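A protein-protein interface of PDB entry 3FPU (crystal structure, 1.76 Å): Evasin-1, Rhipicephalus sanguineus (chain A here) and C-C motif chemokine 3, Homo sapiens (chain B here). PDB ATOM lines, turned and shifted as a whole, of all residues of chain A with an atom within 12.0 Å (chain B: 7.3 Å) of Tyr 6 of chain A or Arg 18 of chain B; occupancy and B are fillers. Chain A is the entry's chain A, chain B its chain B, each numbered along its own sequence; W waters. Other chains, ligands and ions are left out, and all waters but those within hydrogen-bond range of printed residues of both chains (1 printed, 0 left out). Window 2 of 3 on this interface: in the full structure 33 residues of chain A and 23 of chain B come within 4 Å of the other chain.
The backbone NH of Glu 4 of chain A sits at hydrogen-bond distance from the side-chain hydroxyl of Ser 17 of chain B (2.5 Å). The side-chain hydroxyl (OG) of Ser 17 of chain B is in hydrogen-bond range of the backbone NH (N) of Asp 3 of chain A, 2.7 Å away. The backbone carbonyl oxygen (O) of Leu 9 of chain A lies within hydrogen-bond range of the side-chain hydroxyl (OG1) of Thr 16 of chain B, 2.8 Å away. The backbone carbonyl oxygen (O) of Tyr 6 of chain A sits at hydrogen-bond distance from the guanidinium group (NH2) of Arg 18 of chain B (3.5 Å). The backbone NH of Cys 51 of chain B lies within hydrogen-bond range of the backbone carbonyl oxygen of Gly 11 of chain A, at 2.9 Å. The backbone carbonyl oxygen of Asp 2 of chain A lies close to the backbone carbonyl oxygen of Ser 17 of chain B, at 2.9 Å. O of Gly 7 of chain A sits at hydrogen-bond distance from NH2 of Arg 18 of chain B, at 2.9 Å.
The side-chain sulfur of Cys 12 of chain A forms a disulfide with the side-chain sulfur of Cys 33 of chain A (2.0 Å). The side-chain carboxylate (OD2) of Asp 8 of chain A sits at hydrogen-bond distance from the backbone NH (N) of Gly 10 of chain A. N of Thr 16 of chain B is in hydrogen-bond range of O of Cys 51 of chain B (2.8 Å).
Among the printed residues, merely in contact across the chains: Asp 5 of chain A with Arg 18 of chain B (3.2 Å), Gly 11 of chain A with Val 50 of chain B (3.8 Å), Gly 10 of chain A with Val 50 of chain B (3.8 Å), Leu 9 of chain A with Ser 17 of chain B (3.9 Å) and Gly 11 of chain A with Thr 16 of chain B (3.9 Å).
Tyr 6 of chain A touches just one residue of chain B: Arg 18. Of chain A, only Asp 5, Tyr 6 and Gly 7 come within 4 Å of Arg 18 of chain B. Of chain A, only Leu 9 and Gly 11 come within 4 Å of Thr 16 of chain B. Gln 19 of chain B touches none of the printed residues of chain A. Printed residues of chain B within 4 Å of Gly 11 of chain A: Thr 16 (3.9 Å), Val 50 (3.8 Å) and Cys 51 (2.9 Å). Of the printed residues of chain A, Val 50 of chain B touches Gly 10 (3.8 Å) and Gly 11 (3.8 Å). Printed residues of chain B within 4 Å of Gly 10 of chain A: Val 50 (3.8 Å). Of the printed residues of chain B, Asp 3 of chain A touches Ser 17. Printed residues of chain B within 4 Å of Leu 9 of chain A: Thr 16 (2.8 Å) and Ser 17 (3.9 Å). Pro 21 of chain B touches none of the printed residues of chain A. The nearest residue of chain B that does not touch Tyr 6 of chain A is Ser 17 of chain B (6.7 Å). The nearest residue of chain A that does not touch Arg 18 of chain B is Leu 9 of chain A (4.2 Å). The nearest printed residue of chain B that does not touch Gly 11 of chain A is Tyr 15 of chain B (4.1 Å).
Hydrophobic or aromatic side chains of chain A within 4 Å of the printed part of chain B: Tyr 6 and Leu 9. Of the 12 printed residues of chain B, 5 touch a printed residue of chain A. Among the printed residues, no Asp or Glu carboxylate lies within 4 Å of a Lys or Arg side-chain nitrogen of the other chain.
Water W1 lies within hydrogen-bond range of OG of Ser 17 of chain B (2.8 Å), O of Tyr 15 of chain B (3.1 Å) and OE1 of Glu 4 of chain A (3.4 Å).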
ATOM      1  N   GLU A   1     -19.218 -12.537 -15.590  1.00  0.00           N
ATOM      2  CA  GLU A   1     -19.259 -12.181 -17.041  1.00  0.00           C
ATOM      3  C   GLU A   1     -20.592 -11.512 -17.409  1.00  0.00           C
ATOM      4  O   GLU A   1     -21.596 -12.197 -17.652  1.00  0.00           O
ATOM      5  CB  GLU A   1     -18.998 -13.425 -17.903  1.00  0.00           C
ATOM      6  CG  GLU A   1     -18.665 -13.138 -19.373  1.00  0.00           C
ATOM      7  CD  GLU A   1     -19.895 -13.088 -20.279  1.00  0.00           C
ATOM      8  OE1 GLU A   1     -19.853 -12.359 -21.296  1.00  0.00           O
ATOM      9  OE2 GLU A   1     -20.900 -13.776 -19.986  1.00  0.00           O
ATOM     10  N   ASP A   2     -20.579 -10.175 -17.435  1.00  0.00           N
ATOM     11  CA  ASP A   2     -21.745  -9.327 -17.767  1.00  0.00           C
ATOM     12  C   ASP A   2     -22.860  -9.344 -16.708  1.00  0.00           C
ATOM     13  O   ASP A   2     -23.388 -10.410 -16.361  1.00  0.00           O
ATOM     14  CB  ASP A   2     -22.305  -9.660 -19.167  1.00  0.00           C
ATOM     15  N   ASP A   3     -23.225  -8.172 -16.185  1.00  0.00           N
ATOM     16  CA  ASP A   3     -22.605  -6.889 -16.517  1.00  0.00           C
ATOM     17  C   ASP A   3     -21.797  -6.414 -15.305  1.00  0.00           C
ATOM     18  O   ASP A   3     -20.620  -6.029 -15.419  1.00  0.00           O
ATOM     19  CB  ASP A   3     -23.689  -5.853 -16.842  1.00  0.00           C
ATOM     20  CG  ASP A   3     -24.639  -6.297 -17.963  1.00  0.00           C
ATOM     21  OD1 ASP A   3     -24.241  -7.102 -18.835  1.00  0.00           O
ATOM     22  OD2 ASP A   3     -25.795  -5.811 -17.975  1.00  0.00           O
ATOM     23  N   GLU A   4     -22.466  -6.423 -14.152  1.00  0.00           N
ATOM     24  CA  GLU A   4     -21.840  -6.266 -12.851  1.00  0.00           C
ATOM     25  C   GLU A   4     -21.210  -7.605 -12.463  1.00  0.00           C
ATOM     26  O   GLU A   4     -21.779  -8.669 -12.751  1.00  0.00           O
ATOM     27  CB  GLU A   4     -22.886  -5.859 -11.805  1.00  0.00           C
ATOM     28  CG  GLU A   4     -23.419  -4.425 -11.915  1.00  0.00           C
ATOM     29  CD  GLU A   4     -24.542  -4.229 -12.929  1.00  0.00           C
ATOM     30  OE1 GLU A   4     -25.729  -4.229 -12.518  1.00  0.00           O
ATOM     31  OE2 GLU A   4     -24.247  -4.041 -14.129  1.00  0.00           O
ATOM     32  N   ASP A   5     -20.033  -7.569 -11.844  1.00  0.00           N
ATOM     33  CA  ASP A   5     -19.452  -8.800 -11.306  1.00  0.00           C
ATOM     34  C   ASP A   5     -20.021  -9.097  -9.912  1.00  0.00           C
ATOM     35  O   ASP A   5     -20.777 -10.053  -9.757  1.00  0.00           O
ATOM     36  CB  ASP A   5     -17.912  -8.778 -11.308  1.00  0.00           C
ATOM     37  CG  ASP A   5     -17.309  -9.432 -12.552  1.00  0.00           C
ATOM     38  OD1 ASP A   5     -17.396  -8.847 -13.657  1.00  0.00           O
ATOM     39  OD2 ASP A   5     -16.729 -10.534 -12.420  1.00  0.00           O
ATOM     40  N   TYR A   6     -19.704  -8.258  -8.922  1.00  0.00           N
ATOM     41  CA  TYR A   6     -20.076  -8.541  -7.524  1.00  0.00           C
ATOM     42  C   TYR A   6     -20.679  -7.358  -6.747  1.00  0.00           C
ATOM     43  O   TYR A   6     -20.567  -7.288  -5.522  1.00  0.00           O
ATOM     44  CB  TYR A   6     -18.882  -9.117  -6.751  1.00  0.00           C
ATOM     45  CG  TYR A   6     -18.215 -10.340  -7.369  1.00  0.00           C
ATOM     46  CD1 TYR A   6     -18.930 -11.525  -7.606  1.00  0.00           C
ATOM     47  CD2 TYR A   6     -16.857 -10.321  -7.675  1.00  0.00           C
ATOM     48  CE1 TYR A   6     -18.297 -12.654  -8.165  1.00  0.00           C
ATOM     49  CE2 TYR A   6     -16.216 -11.440  -8.221  1.00  0.00           C
ATOM     50  CZ  TYR A   6     -16.939 -12.599  -8.467  1.00  0.00           C
ATOM     51  OH  TYR A   6     -16.284 -13.690  -9.012  1.00  0.00           O
ATOM     52  N   GLY A   7     -21.328  -6.431  -7.445  1.00  0.00           N
ATOM     53  CA  GLY A   7     -22.122  -5.400  -6.760  1.00  0.00           C
ATOM     54  C   GLY A   7     -23.440  -5.948  -6.198  1.00  0.00           C
ATOM     55  O   GLY A   7     -23.598  -7.171  -6.001  1.00  0.00           O
ATOM     56  N   ASP A   8     -24.388  -5.055  -5.930  1.00  0.00           N
ATOM     57  CA  ASP A   8     -25.690  -5.468  -5.399  1.00  0.00           C
ATOM     58  C   ASP A   8     -26.394  -6.301  -6.468  1.00  0.00           C
ATOM     59  O   ASP A   8     -26.167  -6.119  -7.661  1.00  0.00           O
ATOM     60  CB  ASP A   8     -26.552  -4.249  -5.018  1.00  0.00           C
ATOM     61  CG  ASP A   8     -27.958  -4.638  -4.539  1.00  0.00           C
ATOM     62  OD1 ASP A   8     -28.062  -5.377  -3.523  1.00  0.00           O
ATOM     63  OD2 ASP A   8     -28.966  -4.208  -5.174  1.00  0.00           O
ATOM     64  N   LEU A   9     -27.271  -7.191  -6.025  1.00  0.00           N
ATOM     65  CA  LEU A   9     -27.994  -8.073  -6.928  1.00  0.00           C
ATOM     66  C   LEU A   9     -28.765  -7.304  -7.997  1.00  0.00           C
ATOM     67  O   LEU A   9     -28.800  -7.722  -9.154  1.00  0.00           O
ATOM     68  CB  LEU A   9     -28.917  -8.992  -6.132  1.00  0.00           C
ATOM     69  CG  LEU A   9     -28.789 -10.497  -6.384  1.00  0.00           C
ATOM     70  CD1 LEU A   9     -27.325 -10.945  -6.444  1.00  0.00           C
ATOM     71  CD2 LEU A   9     -29.539 -11.266  -5.301  1.00  0.00           C
ATOM     72  N   GLY A  10     -29.344  -6.164  -7.632  1.00  0.00           N
ATOM     73  CA  GLY A  10     -30.084  -5.369  -8.613  1.00  0.00           C
ATOM     74  C   GLY A  10     -31.319  -6.148  -9.060  1.00  0.00           C
ATOM     75  O   GLY A  10     -31.865  -6.924  -8.280  1.00  0.00           O
ATOM     76  N   GLY A  11     -31.726  -5.951 -10.315  1.00  0.00           N
ATOM     77  CA  GLY A  11     -32.939  -6.555 -10.871  1.00  0.00           C
ATOM     78  C   GLY A  11     -34.178  -6.167 -10.094  1.00  0.00           C
ATOM     79  O   GLY A  11     -34.946  -7.042  -9.735  1.00  0.00           O
ATOM     80  N   CYS A  12     -34.375  -4.881  -9.796  1.00  0.00           N
ATOM     81  CA  CYS A  12     -35.564  -4.482  -9.041  1.00  0.00           C
ATOM     82  C   CYS A  12     -36.808  -4.724  -9.899  1.00  0.00           C
ATOM     83  O   CYS A  12     -36.941  -4.140 -10.996  1.00  0.00           O
ATOM     84  CB  CYS A  12     -35.537  -3.010  -8.607  1.00  0.00           C
ATOM     85  SG  CYS A  12     -33.964  -2.417  -7.822  1.00  0.00           S
ATOM     86  N   CYS A  33     -34.161  -1.344  -4.582  1.00  0.00           N
ATOM     87  CA  CYS A  33     -34.021  -2.672  -3.989  1.00  0.00           C
ATOM     88  C   CYS A  33     -32.590  -2.783  -3.463  1.00  0.00           C
ATOM     89  O   CYS A  33     -31.645  -2.590  -4.223  1.00  0.00           O
ATOM     90  CB  CYS A  33     -34.393  -3.756  -5.011  1.00  0.00           C
ATOM     91  SG  CYS A  33     -33.409  -3.887  -6.517  1.00  0.00           S
ATOM     92  N   ASN A  34     -32.430  -3.023  -2.161  1.00  0.00           N
ATOM     93  CA  ASN A  34     -31.092  -2.904  -1.516  1.00  0.00           C
ATOM     94  C   ASN A  34     -30.402  -1.535  -1.770  1.00  0.00           C
ATOM     95  O   ASN A  34     -31.024  -0.488  -1.597  1.00  0.00           O
ATOM     96  CB  ASN A  34     -30.223  -4.072  -1.990  1.00  0.00           C
ATOM     97  CG  ASN A  34     -30.920  -5.429  -1.819  1.00  0.00           C
ATOM     98  OD1 ASN A  34     -30.624  -6.407  -2.535  1.00  0.00           O
ATOM     99  ND2 ASN A  34     -31.868  -5.487  -0.879  1.00  0.00           N
ATOM    100  N   GLY A  35     -29.145  -1.519  -2.203  1.00  0.00           N
ATOM    101  CA  GLY A  35     -28.499  -0.241  -2.602  1.00  0.00           C
ATOM    102  C   GLY A  35     -28.830   0.245  -4.018  1.00  0.00           C
ATOM    103  O   GLY A  35     -28.403   1.326  -4.443  1.00  0.00           O
ATOM    104  N   THR A  36     -29.608  -0.538  -4.760  1.00  0.00           N
ATOM    105  CA  THR A  36     -29.924  -0.198  -6.177  1.00  0.00           C
ATOM    106  C   THR A  36     -31.218   0.591  -6.351  1.00  0.00           C
ATOM    107  O   THR A  36     -32.176   0.408  -5.602  1.00  0.00           O
ATOM    108  CB  THR A  36     -29.961  -1.487  -7.021  1.00  0.00           C
ATOM    109  OG1 THR A  36     -28.688  -2.112  -6.918  1.00  0.00           O
ATOM    110  CG2 THR A  36     -30.296  -1.218  -8.511  1.00  0.00           C
ATOM    111  N   TYR B  15     -32.176  -7.142 -15.422  1.00  0.00           N
ATOM    112  CA  TYR B  15     -32.007  -8.413 -14.763  1.00  0.00           C
ATOM    113  C   TYR B  15     -30.799  -8.364 -13.850  1.00  0.00           C
ATOM    114  O   TYR B  15     -29.892  -7.560 -14.058  1.00  0.00           O
ATOM    115  CB  TYR B  15     -31.815  -9.474 -15.823  1.00  0.00           C
ATOM    116  CG  TYR B  15     -32.884  -9.473 -16.911  1.00  0.00           C
ATOM    117  CD1 TYR B  15     -34.206  -9.784 -16.616  1.00  0.00           C
ATOM    118  CD2 TYR B  15     -32.555  -9.177 -18.244  1.00  0.00           C
ATOM    119  CE1 TYR B  15     -35.198  -9.787 -17.640  1.00  0.00           C
ATOM    120  CE2 TYR B  15     -33.516  -9.208 -19.263  1.00  0.00           C
ATOM    121  CZ  TYR B  15     -34.839  -9.488 -18.949  1.00  0.00           C
ATOM    122  OH  TYR B  15     -35.791  -9.522 -19.955  1.00  0.00           O
ATOM    123  N   THR B  16     -30.807  -9.199 -12.824  1.00  0.00           N
ATOM    124  CA  THR B  16     -29.620  -9.322 -11.983  1.00  0.00           C
ATOM    125  C   THR B  16     -28.391  -9.655 -12.831  1.00  0.00           C
ATOM    126  O   THR B  16     -28.465 -10.366 -13.831  1.00  0.00           O
ATOM    127  CB  THR B  16     -29.809 -10.344 -10.872  1.00  0.00           C
ATOM    128  OG1 THR B  16     -28.610 -10.391 -10.081  1.00  0.00           O
ATOM    129  CG2 THR B  16     -30.107 -11.684 -11.424  1.00  0.00           C
ATOM    130  N   SER B  17     -27.267  -9.092 -12.420  1.00  0.00           N
ATOM    131  CA  SER B  17     -26.045  -9.220 -13.178  1.00  0.00           C
ATOM    132  C   SER B  17     -25.292 -10.514 -12.911  1.00  0.00           C
ATOM    133  O   SER B  17     -24.506 -10.958 -13.753  1.00  0.00           O
ATOM    134  CB  SER B  17     -25.154  -8.043 -12.869  1.00  0.00           C
ATOM    135  OG  SER B  17     -24.726  -7.493 -14.089  1.00  0.00           O
ATOM    136  N   ARG B  18     -25.521 -11.139 -11.763  1.00  0.00           N
ATOM    137  CA  ARG B  18     -24.840 -12.416 -11.531  1.00  0.00           C
ATOM    138  C   ARG B  18     -25.732 -13.592 -11.131  1.00  0.00           C
ATOM    139  O   ARG B  18     -26.862 -13.410 -10.702  1.00  0.00           O
ATOM    140  CB  ARG B  18     -23.689 -12.234 -10.542  1.00  0.00           C
ATOM    141  CG  ARG B  18     -24.127 -11.820  -9.160  1.00  0.00           C
ATOM    142  CD  ARG B  18     -22.962 -11.807  -8.186  1.00  0.00           C
ATOM    143  NE  ARG B  18     -23.154 -10.757  -7.185  1.00  0.00           N
ATOM    144  CZ  ARG B  18     -22.695 -10.808  -5.940  1.00  0.00           C
ATOM    145  NH1 ARG B  18     -22.026 -11.875  -5.517  1.00  0.00           N
ATOM    146  NH2 ARG B  18     -22.922  -9.792  -5.108  1.00  0.00           N
ATOM    147  N   GLN B  19     -25.208 -14.802 -11.299  1.00  0.00           N
ATOM    148  CA  GLN B  19     -25.869 -15.991 -10.816  1.00  0.00           C
ATOM    149  C   GLN B  19     -25.993 -15.990  -9.287  1.00  0.00           C
ATOM    150  O   GLN B  19     -24.995 -15.893  -8.551  1.00  0.00           O
ATOM    151  CB  GLN B  19     -25.139 -17.236 -11.320  1.00  0.00           C
ATOM    152  CG  GLN B  19     -25.916 -18.515 -11.172  1.00  0.00           C
ATOM    153  CD  GLN B  19     -25.220 -19.696 -11.820  1.00  0.00           C
ATOM    154  OE1 GLN B  19     -24.456 -19.535 -12.779  1.00  0.00           O
ATOM    155  NE2 GLN B  19     -25.481 -20.896 -11.298  1.00  0.00           N
ATOM    156  N   ILE B  20     -27.232 -16.086  -8.822  1.00  0.00           N
ATOM    157  CA  ILE B  20     -27.555 -16.127  -7.400  1.00  0.00           C
ATOM    158  C   ILE B  20     -27.226 -17.545  -6.944  1.00  0.00           C
ATOM    159  O   ILE B  20     -27.524 -18.500  -7.682  1.00  0.00           O
ATOM    160  CB  ILE B  20     -29.064 -15.833  -7.176  1.00  0.00           C
ATOM    161  CG1 ILE B  20     -29.434 -14.466  -7.758  1.00  0.00           C
ATOM    162  CG2 ILE B  20     -29.437 -15.904  -5.694  1.00  0.00           C
ATOM    163  CD1 ILE B  20     -30.888 -14.257  -7.828  1.00  0.00           C
ATOM    164  N   PRO B  21     -26.568 -17.704  -5.764  1.00  0.00           N
ATOM    165  CA  PRO B  21     -26.337 -19.069  -5.284  1.00  0.00           C
ATOM    166  C   PRO B  21     -27.617 -19.880  -5.192  1.00  0.00           C
ATOM    167  O   PRO B  21     -28.603 -19.457  -4.558  1.00  0.00           O
ATOM    168  CB  PRO B  21     -25.727 -18.877  -3.877  1.00  0.00           C
ATOM    169  CG  PRO B  21     -25.868 -17.426  -3.571  1.00  0.00           C
ATOM    170  CD  PRO B  21     -25.968 -16.697  -4.866  1.00  0.00           C
ATOM    171  N   VAL B  50     -36.301 -10.848  -7.176  1.00  0.00           N
ATOM    172  CA  VAL B  50     -35.226 -10.392  -8.073  1.00  0.00           C
ATOM    173  C   VAL B  50     -35.510 -10.766  -9.544  1.00  0.00           C
ATOM    174  O   VAL B  50     -35.806 -11.908  -9.827  1.00  0.00           O
ATOM    175  CB  VAL B  50     -33.855 -10.982  -7.676  1.00  0.00           C
ATOM    176  CG1 VAL B  50     -33.898 -12.446  -7.563  1.00  0.00           C
ATOM    177  CG2 VAL B  50     -32.795 -10.554  -8.676  1.00  0.00           C
ATOM    178  N   CYS B  51     -35.420  -9.807 -10.449  1.00  0.00           N
ATOM    179  CA  CYS B  51     -35.563 -10.119 -11.897  1.00  0.00           C
ATOM    180  C   CYS B  51     -34.400 -10.907 -12.485  1.00  0.00           C
ATOM    181  O   CYS B  51     -33.254 -10.535 -12.295  1.00  0.00           O
ATOM    182  CB  CYS B  51     -35.701  -8.842 -12.698  1.00  0.00           C
ATOM    183  SG  CYS B  51     -37.275  -8.068 -12.455  1.00  0.00           S
ATOM    184  N   ALA B  52     -34.699 -11.937 -13.252  1.00  0.00           N
ATOM    185  CA  ALA B  52     -33.679 -12.680 -13.969  1.00  0.00           C
ATOM    186  C   ALA B  52     -34.064 -12.965 -15.432  1.00  0.00           C
ATOM    187  O   ALA B  52     -35.237 -13.011 -15.784  1.00  0.00           O
ATOM    188  CB  ALA B  52     -33.350 -13.958 -13.229  1.00  0.00           C
ATOM    189  N   GLU B  56     -31.175 -17.093 -20.049  1.00  0.00           N
ATOM    190  CA  GLU B  56     -29.931 -17.570 -19.429  1.00  0.00           C
ATOM    191  C   GLU B  56     -30.052 -18.988 -18.903  1.00  0.00           C
ATOM    192  O   GLU B  56     -31.078 -19.368 -18.312  1.00  0.00           O
ATOM    193  CB  GLU B  56     -29.453 -16.624 -18.339  1.00  0.00           C
ATOM    194  CG  GLU B  56     -28.927 -15.306 -18.875  1.00  0.00           C
ATOM    195  CD  GLU B  56     -28.446 -14.403 -17.783  1.00  0.00           C
ATOM    196  OE1 GLU B  56     -28.785 -14.666 -16.614  1.00  0.00           O
ATOM    197  OE2 GLU B  56     -27.718 -13.431 -18.082  1.00  0.00           O
ATOM    198  N   TRP B  58     -28.649 -20.714 -16.470  1.00  0.00           N
ATOM    199  CA  TRP B  58     -28.732 -20.917 -15.017  1.00  0.00           C
ATOM    200  C   TRP B  58     -30.144 -20.684 -14.551  1.00  0.00           C
ATOM    201  O   TRP B  58     -30.614 -21.323 -13.620  1.00  0.00           O
ATOM    202  CB  TRP B  58     -27.754 -20.026 -14.236  1.00  0.00           C
ATOM    203  CG  TRP B  58     -28.033 -18.524 -14.212  1.00  0.00           C
ATOM    204  CD1 TRP B  58     -27.595 -17.598 -15.111  1.00  0.00           C
ATOM    205  CD2 TRP B  58     -28.760 -17.782 -13.204  1.00  0.00           C
ATOM    206  NE1 TRP B  58     -27.990 -16.339 -14.727  1.00  0.00           N
ATOM    207  CE2 TRP B  58     -28.712 -16.427 -13.567  1.00  0.00           C
ATOM    208  CE3 TRP B  58     -29.430 -18.136 -12.038  1.00  0.00           C
ATOM    209  CZ2 TRP B  58     -29.345 -15.425 -12.828  1.00  0.00           C
ATOM    210  CZ3 TRP B  58     -30.048 -17.138 -11.294  1.00  0.00           C
ATOM    211  CH2 TRP B  58     -29.988 -15.797 -11.685  1.00  0.00           C
HETATM  212  O   HOH W   1     -27.160  -6.277 -14.770  1.00  0.00           O
